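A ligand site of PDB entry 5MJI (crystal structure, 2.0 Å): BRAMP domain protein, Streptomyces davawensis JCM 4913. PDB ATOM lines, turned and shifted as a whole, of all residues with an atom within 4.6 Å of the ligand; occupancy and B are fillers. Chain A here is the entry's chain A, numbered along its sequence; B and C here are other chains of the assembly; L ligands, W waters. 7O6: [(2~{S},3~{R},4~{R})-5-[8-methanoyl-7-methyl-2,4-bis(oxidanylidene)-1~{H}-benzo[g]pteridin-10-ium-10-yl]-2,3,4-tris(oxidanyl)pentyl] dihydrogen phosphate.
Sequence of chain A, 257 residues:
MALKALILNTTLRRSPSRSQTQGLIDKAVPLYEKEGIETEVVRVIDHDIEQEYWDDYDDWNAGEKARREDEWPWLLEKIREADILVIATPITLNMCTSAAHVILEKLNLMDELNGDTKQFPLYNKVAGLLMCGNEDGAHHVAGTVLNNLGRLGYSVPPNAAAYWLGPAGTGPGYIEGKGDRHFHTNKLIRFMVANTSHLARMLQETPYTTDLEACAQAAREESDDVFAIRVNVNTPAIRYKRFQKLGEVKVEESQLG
Water W8 bridges O10 of the ligand and NH1 of Arg 13.
Water W3 lies within hydrogen-bond range of an oxygen (O3) of the ligand (2.7 Å), the backbone NH of Leu 12 (2.9 Å) and the side-chain hydroxyl of Thr 11 (3.4 Å).
Water W1 lies within hydrogen-bond range of O5 of the ligand (3.0 Å), OD1 of Asn 134 (3.0 Å) and SG of Cys 132 (3.4 Å).
Water W7 bridges a nitrogen (N2) of the ligand (3.1 Å) and the backbone NH of Leu 93 (3.4 Å).
Pro 90 touches the ligand.
Thr 92 touches the ligand (CA to N2, 3.5 Å).
Gly 133 touches the ligand (C to O9, 3.4 Å).
Tyr 240 of chain B touches the ligand (CE2 to C15, 3.2 Å).
Glu 105 of chain C touches the ligand (O to C11, 3.5 Å).
Asn 108 of chain C touches the ligand (CB to C11, 3.9 Å).
Hydrophobic or aromatic side chains within 4 Å of the ligand: Pro 90, Ile 91 and Tyr 240 of chain B.
Of the 24 residues printed, 18 come within 4 Å of the ligand.
N of Ile 91 is in hydrogen-bond range of O7 of the ligand (3.4 Å).
O of Ile 91 is in hydrogen-bond range of O7 of the ligand.
The side-chain hydroxyl of Ser 19 lies within hydrogen-bond range of an oxygen (O2) of the ligand (2.6 Å).
OG1 of Thr 11 lies within hydrogen-bond range of O3 of the ligand (2.6 Å).
O9 of the ligand lies within hydrogen-bond range of N of Glu 135 (2.7 Å).
The backbone NH (N) of Asp 136 is in hydrogen-bond range of an oxygen (O9) of the ligand (2.7 Å).
O of Asp 136 lies within hydrogen-bond range of N4 of the ligand (2.7 Å).
The backbone NH (N) of Gln 20 is in hydrogen-bond range of an oxygen (O1) of the ligand, 2.7 Å away.
The backbone NH of Asn 94 is in hydrogen-bond range of an oxygen (O8) of the ligand (2.8 Å).
The backbone NH of Asn 134 sits at hydrogen-bond distance from an oxygen (O9) of the ligand (2.9 Å).
The backbone NH (N) of Thr 21 is in hydrogen-bond range of an oxygen (O2) of the ligand, 3.1 Å away.
O2 of the ligand sits at hydrogen-bond distance from OG1 of Thr 21 (3.0 Å).
The guanidinium group (NE) of Arg 13 is in salt-bridge range of an oxygen (O1) of the ligand (3.1 Å).
The backbone carbonyl oxygen of Cys 132 lies within hydrogen-bond range of an oxygen (O5) of the ligand, at 3.1 Å.
The backbone NH (N) of Leu 93 is in hydrogen-bond range of a nitrogen (N2) of the ligand (3.1 Å).
N of Ile 91 is in hydrogen-bond range of O of Cys 132.
The backbone NH of Thr 21 sits at hydrogen-bond distance from the side-chain hydroxyl of Ser 19 (3.2 Å).
The side-chain hydroxyl (OG1) of Thr 11 sits close to the guanidinium group (NE) of Arg 13, at 3.3 Å.
OE1 of Glu 135 lies within hydrogen-bond range of OH of Tyr 240 of chain B, 2.4 Å away.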
ATOM      1  N   THR A  11       3.780  19.225   7.231  1.00  0.00           N
ATOM      2  CA  THR A  11       2.408  19.576   7.571  1.00  0.00           C
ATOM      3  C   THR A  11       2.355  20.915   8.322  1.00  0.00           C
ATOM      4  O   THR A  11       3.296  21.303   9.016  1.00  0.00           O
ATOM      5  CB  THR A  11       1.792  18.471   8.441  1.00  0.00           C
ATOM      6  OG1 THR A  11       0.424  18.775   8.715  1.00  0.00           O
ATOM      7  CG2 THR A  11       2.543  18.331   9.772  1.00  0.00           C
ATOM      8  N   LEU A  12       1.227  21.607   8.178  1.00  0.00           N
ATOM      9  CA  LEU A  12       1.013  22.874   8.876  1.00  0.00           C
ATOM     10  C   LEU A  12       0.501  22.695  10.307  1.00  0.00           C
ATOM     11  O   LEU A  12       0.351  23.706  11.015  1.00  0.00           O
ATOM     12  CB  LEU A  12       0.011  23.748   8.087  1.00  0.00           C
ATOM     13  CG  LEU A  12       0.466  24.128   6.665  1.00  0.00           C
ATOM     14  CD1 LEU A  12      -0.594  24.896   5.903  1.00  0.00           C
ATOM     15  CD2 LEU A  12       1.778  24.913   6.681  1.00  0.00           C
ATOM     16  N   ARG A  13       0.230  21.474  10.749  1.00  0.00           N
ATOM     17  CA  ARG A  13      -0.387  21.238  12.050  1.00  0.00           C
ATOM     18  C   ARG A  13       0.650  20.666  13.023  1.00  0.00           C
ATOM     19  O   ARG A  13       1.361  19.711  12.704  1.00  0.00           O
ATOM     20  CB  ARG A  13      -1.604  20.302  11.922  1.00  0.00           C
ATOM     21  CG  ARG A  13      -1.307  18.874  11.500  1.00  0.00           C
ATOM     22  CD  ARG A  13      -2.558  18.178  10.951  1.00  0.00           C
ATOM     23  NE  ARG A  13      -2.798  18.529   9.554  1.00  0.00           N
ATOM     24  CZ  ARG A  13      -3.751  19.358   9.138  1.00  0.00           C
ATOM     25  NH1 ARG A  13      -3.863  19.632   7.841  1.00  0.00           N
ATOM     26  NH2 ARG A  13      -4.573  19.935  10.011  1.00  0.00           N
ATOM     27  N   ARG A  18      -3.202  14.664  14.159  1.00  0.00           N
ATOM     28  CA  ARG A  18      -3.015  13.604  13.180  1.00  0.00           C
ATOM     29  C   ARG A  18      -2.696  14.206  11.817  1.00  0.00           C
ATOM     30  O   ARG A  18      -3.414  15.076  11.340  1.00  0.00           O
ATOM     31  CB  ARG A  18      -4.282  12.745  13.058  1.00  0.00           C
ATOM     32  CG  ARG A  18      -4.495  11.687  14.115  1.00  0.00           C
ATOM     33  CD  ARG A  18      -5.951  11.192  14.030  1.00  0.00           C
ATOM     34  NE  ARG A  18      -6.880  12.307  14.211  1.00  0.00           N
ATOM     35  CZ  ARG A  18      -8.185  12.268  13.946  1.00  0.00           C
ATOM     36  NH1 ARG A  18      -8.742  11.166  13.459  1.00  0.00           N
ATOM     37  NH2 ARG A  18      -8.950  13.339  14.146  1.00  0.00           N
ATOM     38  N   SER A  19      -1.620  13.740  11.194  1.00  0.00           N
ATOM     39  CA  SER A  19      -1.213  14.227   9.888  1.00  0.00           C
ATOM     40  C   SER A  19      -1.505  13.168   8.832  1.00  0.00           C
ATOM     41  O   SER A  19      -1.092  12.017   8.987  1.00  0.00           O
ATOM     42  CB  SER A  19       0.266  14.600   9.871  1.00  0.00           C
ATOM     43  OG  SER A  19       0.800  14.580   8.561  1.00  0.00           O
ATOM     44  N   GLN A  20      -2.206  13.558   7.763  1.00  0.00           N
ATOM     45  CA  GLN A  20      -2.416  12.619   6.666  1.00  0.00           C
ATOM     46  C   GLN A  20      -1.081  12.163   6.095  1.00  0.00           C
ATOM     47  O   GLN A  20      -0.902  10.980   5.791  1.00  0.00           O
ATOM     48  CB  GLN A  20      -3.269  13.265   5.563  1.00  0.00           C
ATOM     49  CG  GLN A  20      -4.463  14.054   6.082  1.00  0.00           C
ATOM     50  CD  GLN A  20      -5.578  13.162   6.592  1.00  0.00           C
ATOM     51  OE1 GLN A  20      -5.846  12.112   6.019  1.00  0.00           O
ATOM     52  NE2 GLN A  20      -6.247  13.592   7.655  1.00  0.00           N
ATOM     53  N   THR A  21      -0.143  13.087   5.918  1.00  0.00           N
ATOM     54  CA  THR A  21       1.151  12.786   5.318  1.00  0.00           C
ATOM     55  C   THR A  21       1.950  11.800   6.176  1.00  0.00           C
ATOM     56  O   THR A  21       2.696  10.967   5.647  1.00  0.00           O
ATOM     57  CB  THR A  21       1.955  14.071   5.122  1.00  0.00           C
ATOM     58  OG1 THR A  21       1.179  15.026   4.378  1.00  0.00           O
ATOM     59  CG2 THR A  21       3.245  13.778   4.362  1.00  0.00           C
ATOM     60  N   PRO A  90       2.469  17.577   2.521  1.00  0.00           N
ATOM     61  CA  PRO A  90       1.123  17.722   1.955  1.00  0.00           C
ATOM     62  C   PRO A  90       1.182  18.646   0.746  1.00  0.00           C
ATOM     63  O   PRO A  90       2.139  19.394   0.532  1.00  0.00           O
ATOM     64  CB  PRO A  90       0.297  18.348   3.074  1.00  0.00           C
ATOM     65  CG  PRO A  90       1.162  18.373   4.300  1.00  0.00           C
ATOM     66  CD  PRO A  90       2.593  18.208   3.853  1.00  0.00           C
ATOM     67  N   ILE A  91       0.118  18.631  -0.048  1.00  0.00           N
ATOM     68  CA  ILE A  91       0.001  19.520  -1.186  1.00  0.00           C
ATOM     69  C   ILE A  91      -0.911  20.671  -0.816  1.00  0.00           C
ATOM     70  O   ILE A  91      -2.014  20.482  -0.276  1.00  0.00           O
ATOM     71  CB  ILE A  91      -0.511  18.775  -2.426  1.00  0.00           C
ATOM     72  CG1 ILE A  91       0.541  17.741  -2.855  1.00  0.00           C
ATOM     73  CG2 ILE A  91      -0.856  19.797  -3.548  1.00  0.00           C
ATOM     74  CD1 ILE A  91       0.020  16.687  -3.828  1.00  0.00           C
ATOM     75  N   THR A  92      -0.469  21.876  -1.122  1.00  0.00           N
ATOM     76  CA  THR A  92      -1.198  23.069  -0.788  1.00  0.00           C
ATOM     77  C   THR A  92      -1.069  24.029  -1.962  1.00  0.00           C
ATOM     78  O   THR A  92       0.050  24.363  -2.358  1.00  0.00           O
ATOM     79  CB  THR A  92      -0.632  23.598   0.532  1.00  0.00           C
ATOM     80  OG1 THR A  92      -1.556  23.383   1.608  1.00  0.00           O
ATOM     81  CG2 THR A  92      -0.185  24.973   0.436  1.00  0.00           C
ATOM     82  N   LEU A  93      -2.192  24.402  -2.580  1.00  0.00           N
ATOM     83  CA  LEU A  93      -2.194  25.336  -3.727  1.00  0.00           C
ATOM     84  C   LEU A  93      -1.396  24.787  -4.894  1.00  0.00           C
ATOM     85  O   LEU A  93      -0.700  25.533  -5.591  1.00  0.00           O
ATOM     86  CB  LEU A  93      -1.649  26.711  -3.335  1.00  0.00           C
ATOM     87  CG  LEU A  93      -2.016  27.258  -1.966  1.00  0.00           C
ATOM     88  CD1 LEU A  93      -1.166  28.478  -1.640  1.00  0.00           C
ATOM     89  CD2 LEU A  93      -3.503  27.575  -1.959  1.00  0.00           C
ATOM     90  N   ASN A  94      -1.455  23.479  -5.106  1.00  0.00           N
ATOM     91  CA  ASN A  94      -0.697  22.804  -6.150  1.00  0.00           C
ATOM     92  C   ASN A  94       0.802  22.981  -5.941  1.00  0.00           C
ATOM     93  O   ASN A  94       1.578  22.882  -6.904  1.00  0.00           O
ATOM     94  CB  ASN A  94      -1.113  23.291  -7.545  1.00  0.00           C
ATOM     95  CG  ASN A  94      -0.995  22.209  -8.594  1.00  0.00           C
ATOM     96  OD1 ASN A  94      -0.243  22.307  -9.548  1.00  0.00           O
ATOM     97  ND2 ASN A  94      -1.749  21.169  -8.419  1.00  0.00           N
ATOM     98  N   CYS A 132       1.202  14.038  -0.123  1.00  0.00           N
ATOM     99  CA  CYS A 132      -0.170  13.662   0.158  1.00  0.00           C
ATOM    100  C   CYS A 132      -1.073  14.823  -0.243  1.00  0.00           C
ATOM    101  O   CYS A 132      -0.851  15.951   0.208  1.00  0.00           O
ATOM    102  CB  CYS A 132      -0.334  13.357   1.652  1.00  0.00           C
ATOM    103  SG  CYS A 132      -1.765  12.452   1.972  1.00  0.00           S
ATOM    104  N   GLY A 133      -2.075  14.548  -1.078  1.00  0.00           N
ATOM    105  CA  GLY A 133      -3.059  15.553  -1.448  1.00  0.00           C
ATOM    106  C   GLY A 133      -4.440  14.934  -1.458  1.00  0.00           C
ATOM    107  O   GLY A 133      -4.587  13.708  -1.467  1.00  0.00           O
ATOM    108  N   ASN A 134      -5.464  15.781  -1.446  1.00  0.00           N
ATOM    109  CA  ASN A 134      -6.814  15.235  -1.521  1.00  0.00           C
ATOM    110  C   ASN A 134      -7.175  14.801  -2.942  1.00  0.00           C
ATOM    111  O   ASN A 134      -8.021  13.920  -3.102  1.00  0.00           O
ATOM    112  CB  ASN A 134      -7.843  16.252  -1.012  1.00  0.00           C
ATOM    113  CG  ASN A 134      -7.781  16.435   0.512  1.00  0.00           C
ATOM    114  OD1 ASN A 134      -6.916  15.867   1.180  1.00  0.00           O
ATOM    115  ND2 ASN A 134      -8.678  17.262   1.062  1.00  0.00           N
ATOM    116  N   GLU A 135      -6.546  15.369  -3.970  1.00  0.00           N
ATOM    117  CA  GLU A 135      -6.973  15.049  -5.336  1.00  0.00           C
ATOM    118  C   GLU A 135      -5.901  15.230  -6.404  1.00  0.00           C
ATOM    119  O   GLU A 135      -5.924  14.518  -7.399  1.00  0.00           O
ATOM    120  CB  GLU A 135      -8.176  15.929  -5.743  1.00  0.00           C
ATOM    121  CG  GLU A 135      -7.847  17.419  -5.758  1.00  0.00           C
ATOM    122  CD  GLU A 135      -8.794  18.242  -6.615  1.00  0.00           C
ATOM    123  OE1 GLU A 135      -8.706  19.488  -6.556  1.00  0.00           O
ATOM    124  OE2 GLU A 135      -9.618  17.668  -7.358  1.00  0.00           O
ATOM    125  N   ASP A 136      -5.004  16.202  -6.256  1.00  0.00           N
ATOM    126  CA  ASP A 136      -4.235  16.611  -7.420  1.00  0.00           C
ATOM    127  C   ASP A 136      -2.993  17.388  -7.035  1.00  0.00           C
ATOM    128  O   ASP A 136      -3.035  18.207  -6.102  1.00  0.00           O
ATOM    129  CB  ASP A 136      -5.128  17.459  -8.335  1.00  0.00           C
ATOM    130  CG  ASP A 136      -4.440  17.860  -9.632  1.00  0.00           C
ATOM    131  OD1 ASP A 136      -3.667  17.072 -10.194  1.00  0.00           O
ATOM    132  OD2 ASP A 136      -4.657  18.989 -10.080  1.00  0.00           O
ATOM    133  N   LEU A 165      -3.197  10.363  -3.573  1.00  0.00           N
ATOM    134  CA  LEU A 165      -4.214  11.334  -3.966  1.00  0.00           C
ATOM    135  C   LEU A 165      -5.536  10.603  -4.076  1.00  0.00           C
ATOM    136  O   LEU A 165      -5.573   9.445  -4.493  1.00  0.00           O
ATOM    137  CB  LEU A 165      -3.936  11.985  -5.335  1.00  0.00           C
ATOM    138  CG  LEU A 165      -2.561  12.626  -5.558  1.00  0.00           C
ATOM    139  CD1 LEU A 165      -2.382  12.805  -7.047  1.00  0.00           C
ATOM    140  CD2 LEU A 165      -2.471  13.942  -4.818  1.00  0.00           C
ATOM    141  N   TYR B 240     -10.925  22.345   0.338  1.00  0.00           N
ATOM    142  CA  TYR B 240     -10.456  21.014   0.696  1.00  0.00           C
ATOM    143  C   TYR B 240     -10.790  20.659   2.137  1.00  0.00           C
ATOM    144  O   TYR B 240     -10.613  21.468   3.057  1.00  0.00           O
ATOM    145  CB  TYR B 240      -8.944  20.879   0.464  1.00  0.00           C
ATOM    146  CG  TYR B 240      -8.579  20.951  -1.001  1.00  0.00           C
ATOM    147  CD1 TYR B 240      -8.910  19.906  -1.871  1.00  0.00           C
ATOM    148  CD2 TYR B 240      -7.922  22.062  -1.531  1.00  0.00           C
ATOM    149  CE1 TYR B 240      -8.596  19.957  -3.228  1.00  0.00           C
ATOM    150  CE2 TYR B 240      -7.590  22.120  -2.899  1.00  0.00           C
ATOM    151  CZ  TYR B 240      -7.933  21.061  -3.725  1.00  0.00           C
ATOM    152  OH  TYR B 240      -7.615  21.087  -5.066  1.00  0.00           O
ATOM    153  N   ARG B 242      -9.944  17.411   4.523  1.00  0.00           N
ATOM    154  CA  ARG B 242      -9.276  16.120   4.604  1.00  0.00           C
ATOM    155  C   ARG B 242     -10.065  15.126   5.456  1.00  0.00           C
ATOM    156  O   ARG B 242      -9.897  13.912   5.292  1.00  0.00           O
ATOM    157  CB  ARG B 242      -7.856  16.316   5.158  1.00  0.00           C
ATOM    158  CG  ARG B 242      -7.845  16.682   6.629  1.00  0.00           C
ATOM    159  CD  ARG B 242      -6.681  17.573   7.040  1.00  0.00           C
ATOM    160  NE  ARG B 242      -6.755  17.818   8.477  1.00  0.00           N
ATOM    161  CZ  ARG B 242      -7.543  18.731   9.034  1.00  0.00           C
ATOM    162  NH1 ARG B 242      -7.574  18.876  10.361  1.00  0.00           N
ATOM    163  NH2 ARG B 242      -8.299  19.514   8.267  1.00  0.00           N
ATOM    164  N   TYR C  53      -1.793  25.666  11.426  1.00  0.00           N
ATOM    165  CA  TYR C  53      -3.182  25.361  11.126  1.00  0.00           C
ATOM    166  C   TYR C  53      -3.833  24.660  12.300  1.00  0.00           C
ATOM    167  O   TYR C  53      -3.211  23.808  12.944  1.00  0.00           O
ATOM    168  CB  TYR C  53      -3.299  24.460   9.881  1.00  0.00           C
ATOM    169  CG  TYR C  53      -4.716  24.141   9.483  1.00  0.00           C
ATOM    170  CD1 TYR C  53      -5.448  23.144  10.151  1.00  0.00           C
ATOM    171  CD2 TYR C  53      -5.336  24.826   8.447  1.00  0.00           C
ATOM    172  CE1 TYR C  53      -6.761  22.862   9.800  1.00  0.00           C
ATOM    173  CE2 TYR C  53      -6.649  24.539   8.083  1.00  0.00           C
ATOM    174  CZ  TYR C  53      -7.350  23.559   8.758  1.00  0.00           C
ATOM    175  OH  TYR C  53      -8.651  23.276   8.398  1.00  0.00           O
ATOM    176  N   GLU C 105      -2.712  30.279   1.487  1.00  0.00           N
ATOM    177  CA  GLU C 105      -3.198  29.155   2.294  1.00  0.00           C
ATOM    178  C   GLU C 105      -4.337  29.598   3.201  1.00  0.00           C
ATOM    179  O   GLU C 105      -5.391  28.953   3.274  1.00  0.00           O
ATOM    180  CB  GLU C 105      -2.051  28.565   3.130  1.00  0.00           C
ATOM    181  CG  GLU C 105      -1.181  27.549   2.407  1.00  0.00           C
ATOM    182  CD  GLU C 105       0.088  27.179   3.186  1.00  0.00           C
ATOM    183  OE1 GLU C 105       0.415  27.845   4.198  1.00  0.00           O
ATOM    184  OE2 GLU C 105       0.776  26.203   2.801  1.00  0.00           O
ATOM    185  N   ASN C 108      -7.518  30.485   1.384  1.00  0.00           N
ATOM    186  CA  ASN C 108      -8.229  29.304   0.913  1.00  0.00           C
ATOM    187  C   ASN C 108      -8.984  28.576   2.030  1.00  0.00           C
ATOM    188  O   ASN C 108      -9.580  27.526   1.752  1.00  0.00           O
ATOM    189  CB  ASN C 108      -7.241  28.348   0.221  1.00  0.00           C
ATOM    190  CG  ASN C 108      -7.050  28.685  -1.272  1.00  0.00           C
ATOM    191  OD1 ASN C 108      -7.631  28.037  -2.128  1.00  0.00           O
ATOM    192  ND2 ASN C 108      -6.234  29.689  -1.566  1.00  0.00           N
ATOM    193  N   LEU C 109      -8.981  29.099   3.243  1.00  0.00           N
ATOM    194  CA  LEU C 109      -9.730  28.522   4.359  1.00  0.00           C
ATOM    195  C   LEU C 109     -11.146  29.068   4.491  1.00  0.00           C
ATOM    196  O   LEU C 109     -11.902  28.566   5.325  1.00  0.00           O
ATOM    197  CB  LEU C 109      -9.008  28.749   5.683  1.00  0.00           C
ATOM    198  CG  LEU C 109      -7.611  28.136   5.726  1.00  0.00           C
ATOM    199  CD1 LEU C 109      -6.957  28.366   7.076  1.00  0.00           C
ATOM    200  CD2 LEU C 109      -7.713  26.646   5.393  1.00  0.00           C
HETATM  201  C6  7O6 L   1      -5.158  21.654   0.397  1.00  0.00           C
HETATM  202  C5  7O6 L   1      -5.595  19.223   0.758  1.00  0.00           C
HETATM  203  C4  7O6 L   1      -4.429  18.340   1.282  1.00  0.00           C
HETATM  204  C3  7O6 L   1      -4.167  18.454   2.777  1.00  0.00           C
HETATM  205  C2  7O6 L   1      -3.759  17.097   3.314  1.00  0.00           C
HETATM  206  C1  7O6 L   1      -3.164  17.404   4.679  1.00  0.00           C
HETATM  207  O1  7O6 L   1      -2.496  16.249   7.530  1.00  0.00           O
HETATM  208  P1  7O6 L   1      -1.564  16.761   6.529  1.00  0.00           P
HETATM  209  O2  7O6 L   1      -0.315  16.037   6.727  1.00  0.00           O
HETATM  210  O3  7O6 L   1      -1.339  18.169   6.836  1.00  0.00           O
HETATM  211  O4  7O6 L   1      -2.143  16.532   5.007  1.00  0.00           O
HETATM  212  O5  7O6 L   1      -2.794  16.465   2.525  1.00  0.00           O
HETATM  213  O6  7O6 L   1      -5.222  18.953   3.560  1.00  0.00           O
HETATM  214  O7  7O6 L   1      -3.153  18.537   0.703  1.00  0.00           O
HETATM  215  N1  7O6 L   1      -5.205  20.340  -0.107  1.00  0.00           N
HETATM  216  C7  7O6 L   1      -5.448  21.924   1.721  1.00  0.00           C
HETATM  217  C8  7O6 L   1      -5.380  23.238   2.171  1.00  0.00           C
HETATM  218  C9  7O6 L   1      -5.696  23.536   3.638  1.00  0.00           C
HETATM  219  C10 7O6 L   1      -5.018  24.300   1.349  1.00  0.00           C
HETATM  220  C11 7O6 L   1      -4.937  25.737   1.913  1.00  0.00           C
HETATM  221  C12 7O6 L   1      -4.722  24.028   0.033  1.00  0.00           C
HETATM  222  C13 7O6 L   1      -4.787  22.707  -0.460  1.00  0.00           C
HETATM  223  N2  7O6 L   1      -4.487  22.520  -1.769  1.00  0.00           N
HETATM  224  C14 7O6 L   1      -4.921  20.134  -1.461  1.00  0.00           C
HETATM  225  N3  7O6 L   1      -4.989  18.873  -1.922  1.00  0.00           N
HETATM  226  C15 7O6 L   1      -4.558  21.240  -2.245  1.00  0.00           C
HETATM  227  C16 7O6 L   1      -4.222  21.007  -3.684  1.00  0.00           C
HETATM  228  O8  7O6 L   1      -3.834  22.040  -4.519  1.00  0.00           O
HETATM  229  N4  7O6 L   1      -4.286  19.695  -4.187  1.00  0.00           N
HETATM  230  C17 7O6 L   1      -4.678  18.616  -3.335  1.00  0.00           C
HETATM  231  O9  7O6 L   1      -4.767  17.334  -3.825  1.00  0.00           O
HETATM  232  O10 7O6 L   1      -5.489  22.677   4.435  1.00  0.00           O
HETATM  233  O   HOH W   1      -4.683  14.142   2.235  1.00  0.00           O
HETATM  234  O   HOH W   2      -2.881  21.187   4.433  1.00  0.00           O
HETATM  235  O   HOH W   3      -0.679  20.726   6.113  1.00  0.00           O
HETATM  236  O   HOH W   4      -8.880  23.939   3.043  1.00  0.00           O
HETATM  237  O   HOH W   5      -4.753  15.799   9.037  1.00  0.00           O
HETATM  238  O   HOH W   6      -4.519  26.720   5.037  1.00  0.00           O
HETATM  239  O   HOH W   7      -5.370  24.680  -3.762  1.00  0.00           O
HETATM  240  O   HOH W   8      -5.617  21.423   6.779  1.00  0.00           O
